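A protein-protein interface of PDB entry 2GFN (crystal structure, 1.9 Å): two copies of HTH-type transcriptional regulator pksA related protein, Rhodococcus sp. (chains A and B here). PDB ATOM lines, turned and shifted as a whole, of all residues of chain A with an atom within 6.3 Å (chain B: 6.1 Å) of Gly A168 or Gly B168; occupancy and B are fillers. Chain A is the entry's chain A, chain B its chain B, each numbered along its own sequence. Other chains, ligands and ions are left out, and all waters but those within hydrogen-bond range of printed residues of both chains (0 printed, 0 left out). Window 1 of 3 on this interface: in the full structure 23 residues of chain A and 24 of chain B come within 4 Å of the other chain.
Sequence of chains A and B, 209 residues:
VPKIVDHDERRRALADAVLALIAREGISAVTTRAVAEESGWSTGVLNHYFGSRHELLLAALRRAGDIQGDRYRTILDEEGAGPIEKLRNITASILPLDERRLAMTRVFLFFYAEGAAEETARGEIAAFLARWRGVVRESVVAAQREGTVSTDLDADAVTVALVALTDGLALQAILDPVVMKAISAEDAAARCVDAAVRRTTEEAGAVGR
The side-chain amide nitrogen (NE2) of Gln B172 lies within hydrogen-bond range of the side-chain carboxylate (OD2) of Asp A167 (3.2 Å).
NE2 of Gln A172 lies within hydrogen-bond range of OD2 of Asp B167.
Among the printed residues, merely in contact across the chains: Val A163 with Gln B172 (3.7 Å), Ala A164 with Ala B164 (3.8 Å), Ala A164 with Gly B168 (3.3 Å), Ala A164 with Leu B169 (3.6 Å), Ala A164 with Gln B172 (3.9 Å), Leu A165 with Leu B165 (3.9 Å), Gly A168 with Ala B164 (3.4 Å), Gly A168 with Gly B168 (3.9 Å), Leu A169 with Ala B164 (3.5 Å), Gln A172 with Val B163 (3.8 Å) and Gln A172 with Ala B164 (3.9 Å).
Gly A168 touches just these residues of chain B: Ala B164 and Gly B168.
Gly B168 touches just these residues of chain A: Ala A164 and Gly A168.
Of the printed residues of chain A, Ala B164 touches Ala A164, Gly A168, Leu A169 and Gln A172.
Of the printed residues of chain A, Gln B172 touches Val A163 (3.7 Å), Ala A164 (3.9 Å) and Asp A167 (3.2 Å).
The nearest residue of chain B that does not touch Gly A168 is Asp B167 (4.9 Å).
The nearest residue of chain A that does not touch Gly B168 is Asp A167 (4.9 Å).
The nearest printed residue of chain B that does not touch Leu A169 is Leu B165 (5.9 Å).
Hydrophobic or aromatic side chains of chain B that line the printed part of chain A: Val B163, Ala B164, Leu B165 and Leu B169.
Printed residues of chain A that touch a printed residue of chain B: Val A163, Ala A164, Leu A165, Asp A167, Gly A168, Leu A169 and Gln A172.
Among the printed residues, 13 pairs touch across the chains.
Among the printed residues, no Asp or Glu carboxylate lies within 4 Å of a Lys or Arg side-chain nitrogen of the other chain.
Val A163 touches Gln B172, and with the chains exchanged Gln A172 touches Val B163.
Ala A164 touches Gln B172, and with the chains exchanged Gln A172 touches Ala B164.
Leu A165 touches its own counterpart, Leu B165.
Asp A167 touches Gln B172, and with the chains exchanged Gln A172 touches Asp B167.
Of the 13 pairs that touch across the chains among the printed residues, 13 have their exchanged pair printed and touching as well.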
ATOM      1  N   VAL A 163      30.833 -12.321 -22.838  1.00  0.00           N
ATOM      2  CA  VAL A 163      31.432 -12.879 -21.619  1.00  0.00           C
ATOM      3  C   VAL A 163      30.582 -14.010 -21.081  1.00  0.00           C
ATOM      4  O   VAL A 163      31.119 -15.048 -20.717  1.00  0.00           O
ATOM      5  CB  VAL A 163      31.782 -11.742 -20.577  1.00  0.00           C
ATOM      6  CG1 VAL A 163      32.105 -12.288 -19.201  1.00  0.00           C
ATOM      7  CG2 VAL A 163      32.963 -10.891 -21.135  1.00  0.00           C
ATOM      8  N   ALA A 164      29.260 -13.842 -21.100  1.00  0.00           N
ATOM      9  CA  ALA A 164      28.393 -14.894 -20.603  1.00  0.00           C
ATOM     10  C   ALA A 164      28.469 -16.145 -21.514  1.00  0.00           C
ATOM     11  O   ALA A 164      28.517 -17.268 -21.033  1.00  0.00           O
ATOM     12  CB  ALA A 164      26.955 -14.390 -20.516  1.00  0.00           C
ATOM     13  N   LEU A 165      28.453 -15.937 -22.812  1.00  0.00           N
ATOM     14  CA  LEU A 165      28.523 -17.056 -23.762  1.00  0.00           C
ATOM     15  C   LEU A 165      29.844 -17.794 -23.593  1.00  0.00           C
ATOM     16  O   LEU A 165      29.883 -19.039 -23.544  1.00  0.00           O
ATOM     17  CB  LEU A 165      28.388 -16.514 -25.195  1.00  0.00           C
ATOM     18  CG  LEU A 165      28.729 -17.452 -26.377  1.00  0.00           C
ATOM     19  CD1 LEU A 165      27.832 -18.692 -26.496  1.00  0.00           C
ATOM     20  CD2 LEU A 165      28.610 -16.632 -27.659  1.00  0.00           C
ATOM     21  N   THR A 166      30.923 -17.029 -23.509  1.00  0.00           N
ATOM     22  CA  THR A 166      32.265 -17.620 -23.446  1.00  0.00           C
ATOM     23  C   THR A 166      32.372 -18.436 -22.150  1.00  0.00           C
ATOM     24  O   THR A 166      32.921 -19.536 -22.148  1.00  0.00           O
ATOM     25  CB  THR A 166      33.374 -16.568 -23.431  1.00  0.00           C
ATOM     26  OG1 THR A 166      33.239 -15.674 -24.545  1.00  0.00           O
ATOM     27  CG2 THR A 166      34.768 -17.264 -23.541  1.00  0.00           C
ATOM     28  N   ASP A 167      31.866 -17.885 -21.038  1.00  0.00           N
ATOM     29  CA  ASP A 167      32.007 -18.534 -19.754  1.00  0.00           C
ATOM     30  C   ASP A 167      31.103 -19.770 -19.711  1.00  0.00           C
ATOM     31  O   ASP A 167      31.524 -20.792 -19.180  1.00  0.00           O
ATOM     32  CB  ASP A 167      31.669 -17.551 -18.617  1.00  0.00           C
ATOM     33  CG  ASP A 167      32.444 -17.824 -17.341  1.00  0.00           C
ATOM     34  OD1 ASP A 167      33.418 -18.590 -17.387  1.00  0.00           O
ATOM     35  OD2 ASP A 167      32.076 -17.263 -16.287  1.00  0.00           O
ATOM     36  N   GLY A 168      29.868 -19.677 -20.237  1.00  0.00           N
ATOM     37  CA  GLY A 168      29.000 -20.867 -20.365  1.00  0.00           C
ATOM     38  C   GLY A 168      29.692 -21.976 -21.140  1.00  0.00           C
ATOM     39  O   GLY A 168      29.637 -23.139 -20.735  1.00  0.00           O
ATOM     40  N   LEU A 169      30.362 -21.625 -22.244  1.00  0.00           N
ATOM     41  CA  LEU A 169      31.052 -22.619 -23.044  1.00  0.00           C
ATOM     42  C   LEU A 169      32.220 -23.224 -22.291  1.00  0.00           C
ATOM     43  O   LEU A 169      32.432 -24.464 -22.297  1.00  0.00           O
ATOM     44  CB  LEU A 169      31.580 -22.016 -24.384  1.00  0.00           C
ATOM     45  CG  LEU A 169      30.504 -21.765 -25.458  1.00  0.00           C
ATOM     46  CD1 LEU A 169      31.104 -21.019 -26.594  1.00  0.00           C
ATOM     47  CD2 LEU A 169      29.840 -23.086 -25.996  1.00  0.00           C
ATOM     48  N   ALA A 170      33.008 -22.353 -21.669  1.00  0.00           N
ATOM     49  CA  ALA A 170      34.188 -22.836 -20.923  1.00  0.00           C
ATOM     50  C   ALA A 170      33.742 -23.807 -19.804  1.00  0.00           C
ATOM     51  O   ALA A 170      34.349 -24.883 -19.608  1.00  0.00           O
ATOM     52  CB  ALA A 170      34.945 -21.664 -20.360  1.00  0.00           C
ATOM     53  N   LEU A 171      32.682 -23.431 -19.072  1.00  0.00           N
ATOM     54  CA  LEU A 171      32.257 -24.222 -17.918  1.00  0.00           C
ATOM     55  C   LEU A 171      31.619 -25.530 -18.328  1.00  0.00           C
ATOM     56  O   LEU A 171      31.947 -26.570 -17.732  1.00  0.00           O
ATOM     57  CB  LEU A 171      31.329 -23.441 -16.945  1.00  0.00           C
ATOM     58  CG  LEU A 171      31.919 -22.144 -16.355  1.00  0.00           C
ATOM     59  CD1 LEU A 171      30.879 -21.406 -15.518  1.00  0.00           C
ATOM     60  CD2 LEU A 171      33.176 -22.384 -15.494  1.00  0.00           C
ATOM     61  N   GLN A 172      30.718 -25.495 -19.320  1.00  0.00           N
ATOM     62  CA  GLN A 172      30.092 -26.722 -19.834  1.00  0.00           C
ATOM     63  C   GLN A 172      31.146 -27.630 -20.433  1.00  0.00           C
ATOM     64  O   GLN A 172      31.058 -28.876 -20.335  1.00  0.00           O
ATOM     65  CB  GLN A 172      29.018 -26.396 -20.866  1.00  0.00           C
ATOM     66  CG  GLN A 172      27.775 -25.734 -20.217  1.00  0.00           C
ATOM     67  CD  GLN A 172      26.714 -25.336 -21.227  1.00  0.00           C
ATOM     68  OE1 GLN A 172      26.856 -25.569 -22.434  1.00  0.00           O
ATOM     69  NE2 GLN A 172      25.657 -24.731 -20.747  1.00  0.00           N
ATOM     70  N   ALA A 173      32.142 -27.026 -21.063  1.00  0.00           N
ATOM     71  CA  ALA A 173      33.130 -27.843 -21.760  1.00  0.00           C
ATOM     72  C   ALA A 173      33.881 -28.774 -20.816  1.00  0.00           C
ATOM     73  O   ALA A 173      34.259 -29.862 -21.253  1.00  0.00           O
ATOM     74  CB  ALA A 173      34.099 -26.999 -22.605  1.00  0.00           C
ATOM     75  N   VAL A 179      30.277 -30.175 -25.693  1.00  0.00           N
ATOM     76  CA  VAL A 179      30.669 -28.778 -25.746  1.00  0.00           C
ATOM     77  C   VAL A 179      32.197 -28.680 -25.881  1.00  0.00           C
ATOM     78  O   VAL A 179      32.701 -27.785 -26.555  1.00  0.00           O
ATOM     79  CB  VAL A 179      30.196 -28.015 -24.489  1.00  0.00           C
ATOM     80  CG1 VAL A 179      30.599 -26.521 -24.557  1.00  0.00           C
ATOM     81  CG2 VAL A 179      28.681 -28.164 -24.285  1.00  0.00           C
ATOM     82  N   VAL B 163      22.207 -22.397 -25.609  1.00  0.00           N
ATOM     83  CA  VAL B 163      22.254 -23.024 -24.284  1.00  0.00           C
ATOM     84  C   VAL B 163      23.456 -22.503 -23.479  1.00  0.00           C
ATOM     85  O   VAL B 163      23.333 -22.222 -22.295  1.00  0.00           O
ATOM     86  CB  VAL B 163      22.242 -24.591 -24.416  1.00  0.00           C
ATOM     87  CG1 VAL B 163      22.605 -25.304 -23.099  1.00  0.00           C
ATOM     88  CG2 VAL B 163      20.851 -25.047 -24.860  1.00  0.00           C
ATOM     89  N   ALA B 164      24.610 -22.336 -24.120  1.00  0.00           N
ATOM     90  CA  ALA B 164      25.788 -21.841 -23.374  1.00  0.00           C
ATOM     91  C   ALA B 164      25.599 -20.383 -22.914  1.00  0.00           C
ATOM     92  O   ALA B 164      26.011 -20.019 -21.807  1.00  0.00           O
ATOM     93  CB  ALA B 164      27.011 -21.929 -24.232  1.00  0.00           C
ATOM     94  N   LEU B 165      25.057 -19.552 -23.802  1.00  0.00           N
ATOM     95  CA  LEU B 165      24.763 -18.154 -23.461  1.00  0.00           C
ATOM     96  C   LEU B 165      23.770 -18.092 -22.306  1.00  0.00           C
ATOM     97  O   LEU B 165      23.958 -17.341 -21.310  1.00  0.00           O
ATOM     98  CB  LEU B 165      24.236 -17.371 -24.688  1.00  0.00           C
ATOM     99  CG  LEU B 165      23.730 -15.928 -24.469  1.00  0.00           C
ATOM    100  CD1 LEU B 165      24.823 -15.025 -23.850  1.00  0.00           C
ATOM    101  CD2 LEU B 165      23.133 -15.357 -25.798  1.00  0.00           C
ATOM    102  N   THR B 166      22.699 -18.867 -22.435  1.00  0.00           N
ATOM    103  CA  THR B 166      21.647 -18.799 -21.413  1.00  0.00           C
ATOM    104  C   THR B 166      22.244 -19.251 -20.093  1.00  0.00           C
ATOM    105  O   THR B 166      22.012 -18.651 -19.059  1.00  0.00           O
ATOM    106  CB  THR B 166      20.477 -19.719 -21.767  1.00  0.00           C
ATOM    107  OG1 THR B 166      19.972 -19.399 -23.080  1.00  0.00           O
ATOM    108  CG2 THR B 166      19.413 -19.578 -20.752  1.00  0.00           C
ATOM    109  N   ASP B 167      23.033 -20.321 -20.123  1.00  0.00           N
ATOM    110  CA  ASP B 167      23.575 -20.881 -18.880  1.00  0.00           C
ATOM    111  C   ASP B 167      24.618 -19.935 -18.290  1.00  0.00           C
ATOM    112  O   ASP B 167      24.680 -19.762 -17.051  1.00  0.00           O
ATOM    113  CB  ASP B 167      24.151 -22.290 -19.182  1.00  0.00           C
ATOM    114  CG  ASP B 167      24.296 -23.170 -17.936  1.00  0.00           C
ATOM    115  OD1 ASP B 167      23.563 -22.957 -16.953  1.00  0.00           O
ATOM    116  OD2 ASP B 167      25.143 -24.099 -17.978  1.00  0.00           O
ATOM    117  N   GLY B 168      25.467 -19.342 -19.142  1.00  0.00           N
ATOM    118  CA  GLY B 168      26.489 -18.353 -18.657  1.00  0.00           C
ATOM    119  C   GLY B 168      25.820 -17.178 -17.951  1.00  0.00           C
ATOM    120  O   GLY B 168      26.270 -16.712 -16.888  1.00  0.00           O
ATOM    121  N   LEU B 169      24.713 -16.713 -18.522  1.00  0.00           N
ATOM    122  CA  LEU B 169      23.989 -15.599 -17.939  1.00  0.00           C
ATOM    123  C   LEU B 169      23.342 -16.008 -16.599  1.00  0.00           C
ATOM    124  O   LEU B 169      23.437 -15.253 -15.621  1.00  0.00           O
ATOM    125  CB  LEU B 169      22.919 -15.058 -18.898  1.00  0.00           C
ATOM    126  CG  LEU B 169      23.347 -14.245 -20.150  1.00  0.00           C
ATOM    127  CD1 LEU B 169      22.191 -14.230 -21.188  1.00  0.00           C
ATOM    128  CD2 LEU B 169      23.786 -12.807 -19.789  1.00  0.00           C
ATOM    129  N   ALA B 170      22.691 -17.172 -16.562  1.00  0.00           N
ATOM    130  CA  ALA B 170      22.060 -17.640 -15.317  1.00  0.00           C
ATOM    131  C   ALA B 170      23.091 -17.831 -14.182  1.00  0.00           C
ATOM    132  O   ALA B 170      22.880 -17.428 -13.039  1.00  0.00           O
ATOM    133  CB  ALA B 170      21.249 -18.907 -15.576  1.00  0.00           C
ATOM    134  N   LEU B 171      24.233 -18.429 -14.497  1.00  0.00           N
ATOM    135  CA  LEU B 171      25.231 -18.660 -13.461  1.00  0.00           C
ATOM    136  C   LEU B 171      25.870 -17.363 -12.976  1.00  0.00           C
ATOM    137  O   LEU B 171      26.109 -17.172 -11.766  1.00  0.00           O
ATOM    138  CB  LEU B 171      26.272 -19.653 -13.963  1.00  0.00           C
ATOM    139  CG  LEU B 171      25.716 -21.038 -14.358  1.00  0.00           C
ATOM    140  CD1 LEU B 171      26.788 -21.903 -15.039  1.00  0.00           C
ATOM    141  CD2 LEU B 171      25.086 -21.812 -13.153  1.00  0.00           C
ATOM    142  N   GLN B 172      26.154 -16.464 -13.919  1.00  0.00           N
ATOM    143  CA  GLN B 172      26.743 -15.175 -13.573  1.00  0.00           C
ATOM    144  C   GLN B 172      25.767 -14.321 -12.772  1.00  0.00           C
ATOM    145  O   GLN B 172      26.175 -13.665 -11.784  1.00  0.00           O
ATOM    146  CB  GLN B 172      27.253 -14.428 -14.820  1.00  0.00           C
ATOM    147  CG  GLN B 172      28.509 -15.092 -15.425  1.00  0.00           C
ATOM    148  CD  GLN B 172      29.092 -14.312 -16.588  1.00  0.00           C
ATOM    149  OE1 GLN B 172      28.557 -13.275 -16.953  1.00  0.00           O
ATOM    150  NE2 GLN B 172      30.187 -14.828 -17.184  1.00  0.00           N
ATOM    151  N   ALA B 173      24.492 -14.329 -13.176  1.00  0.00           N
ATOM    152  CA  ALA B 173      23.428 -13.628 -12.438  1.00  0.00           C
ATOM    153  C   ALA B 173      23.355 -13.895 -10.930  1.00  0.00           C
ATOM    154  O   ALA B 173      23.055 -12.968 -10.144  1.00  0.00           O
ATOM    155  CB  ALA B 173      22.081 -13.886 -13.048  1.00  0.00           C
ATOM    156  N   VAL B 179      24.532  -8.422 -13.930  1.00  0.00           N
ATOM    157  CA  VAL B 179      24.016  -9.471 -14.818  1.00  0.00           C
ATOM    158  C   VAL B 179      22.590  -9.813 -14.393  1.00  0.00           C
ATOM    159  O   VAL B 179      21.699  -9.892 -15.236  1.00  0.00           O
ATOM    160  CB  VAL B 179      24.904 -10.742 -14.879  1.00  0.00           C
ATOM    161  CG1 VAL B 179      24.253 -11.792 -15.860  1.00  0.00           C
ATOM    162  CG2 VAL B 179      26.292 -10.380 -15.365  1.00  0.00           C
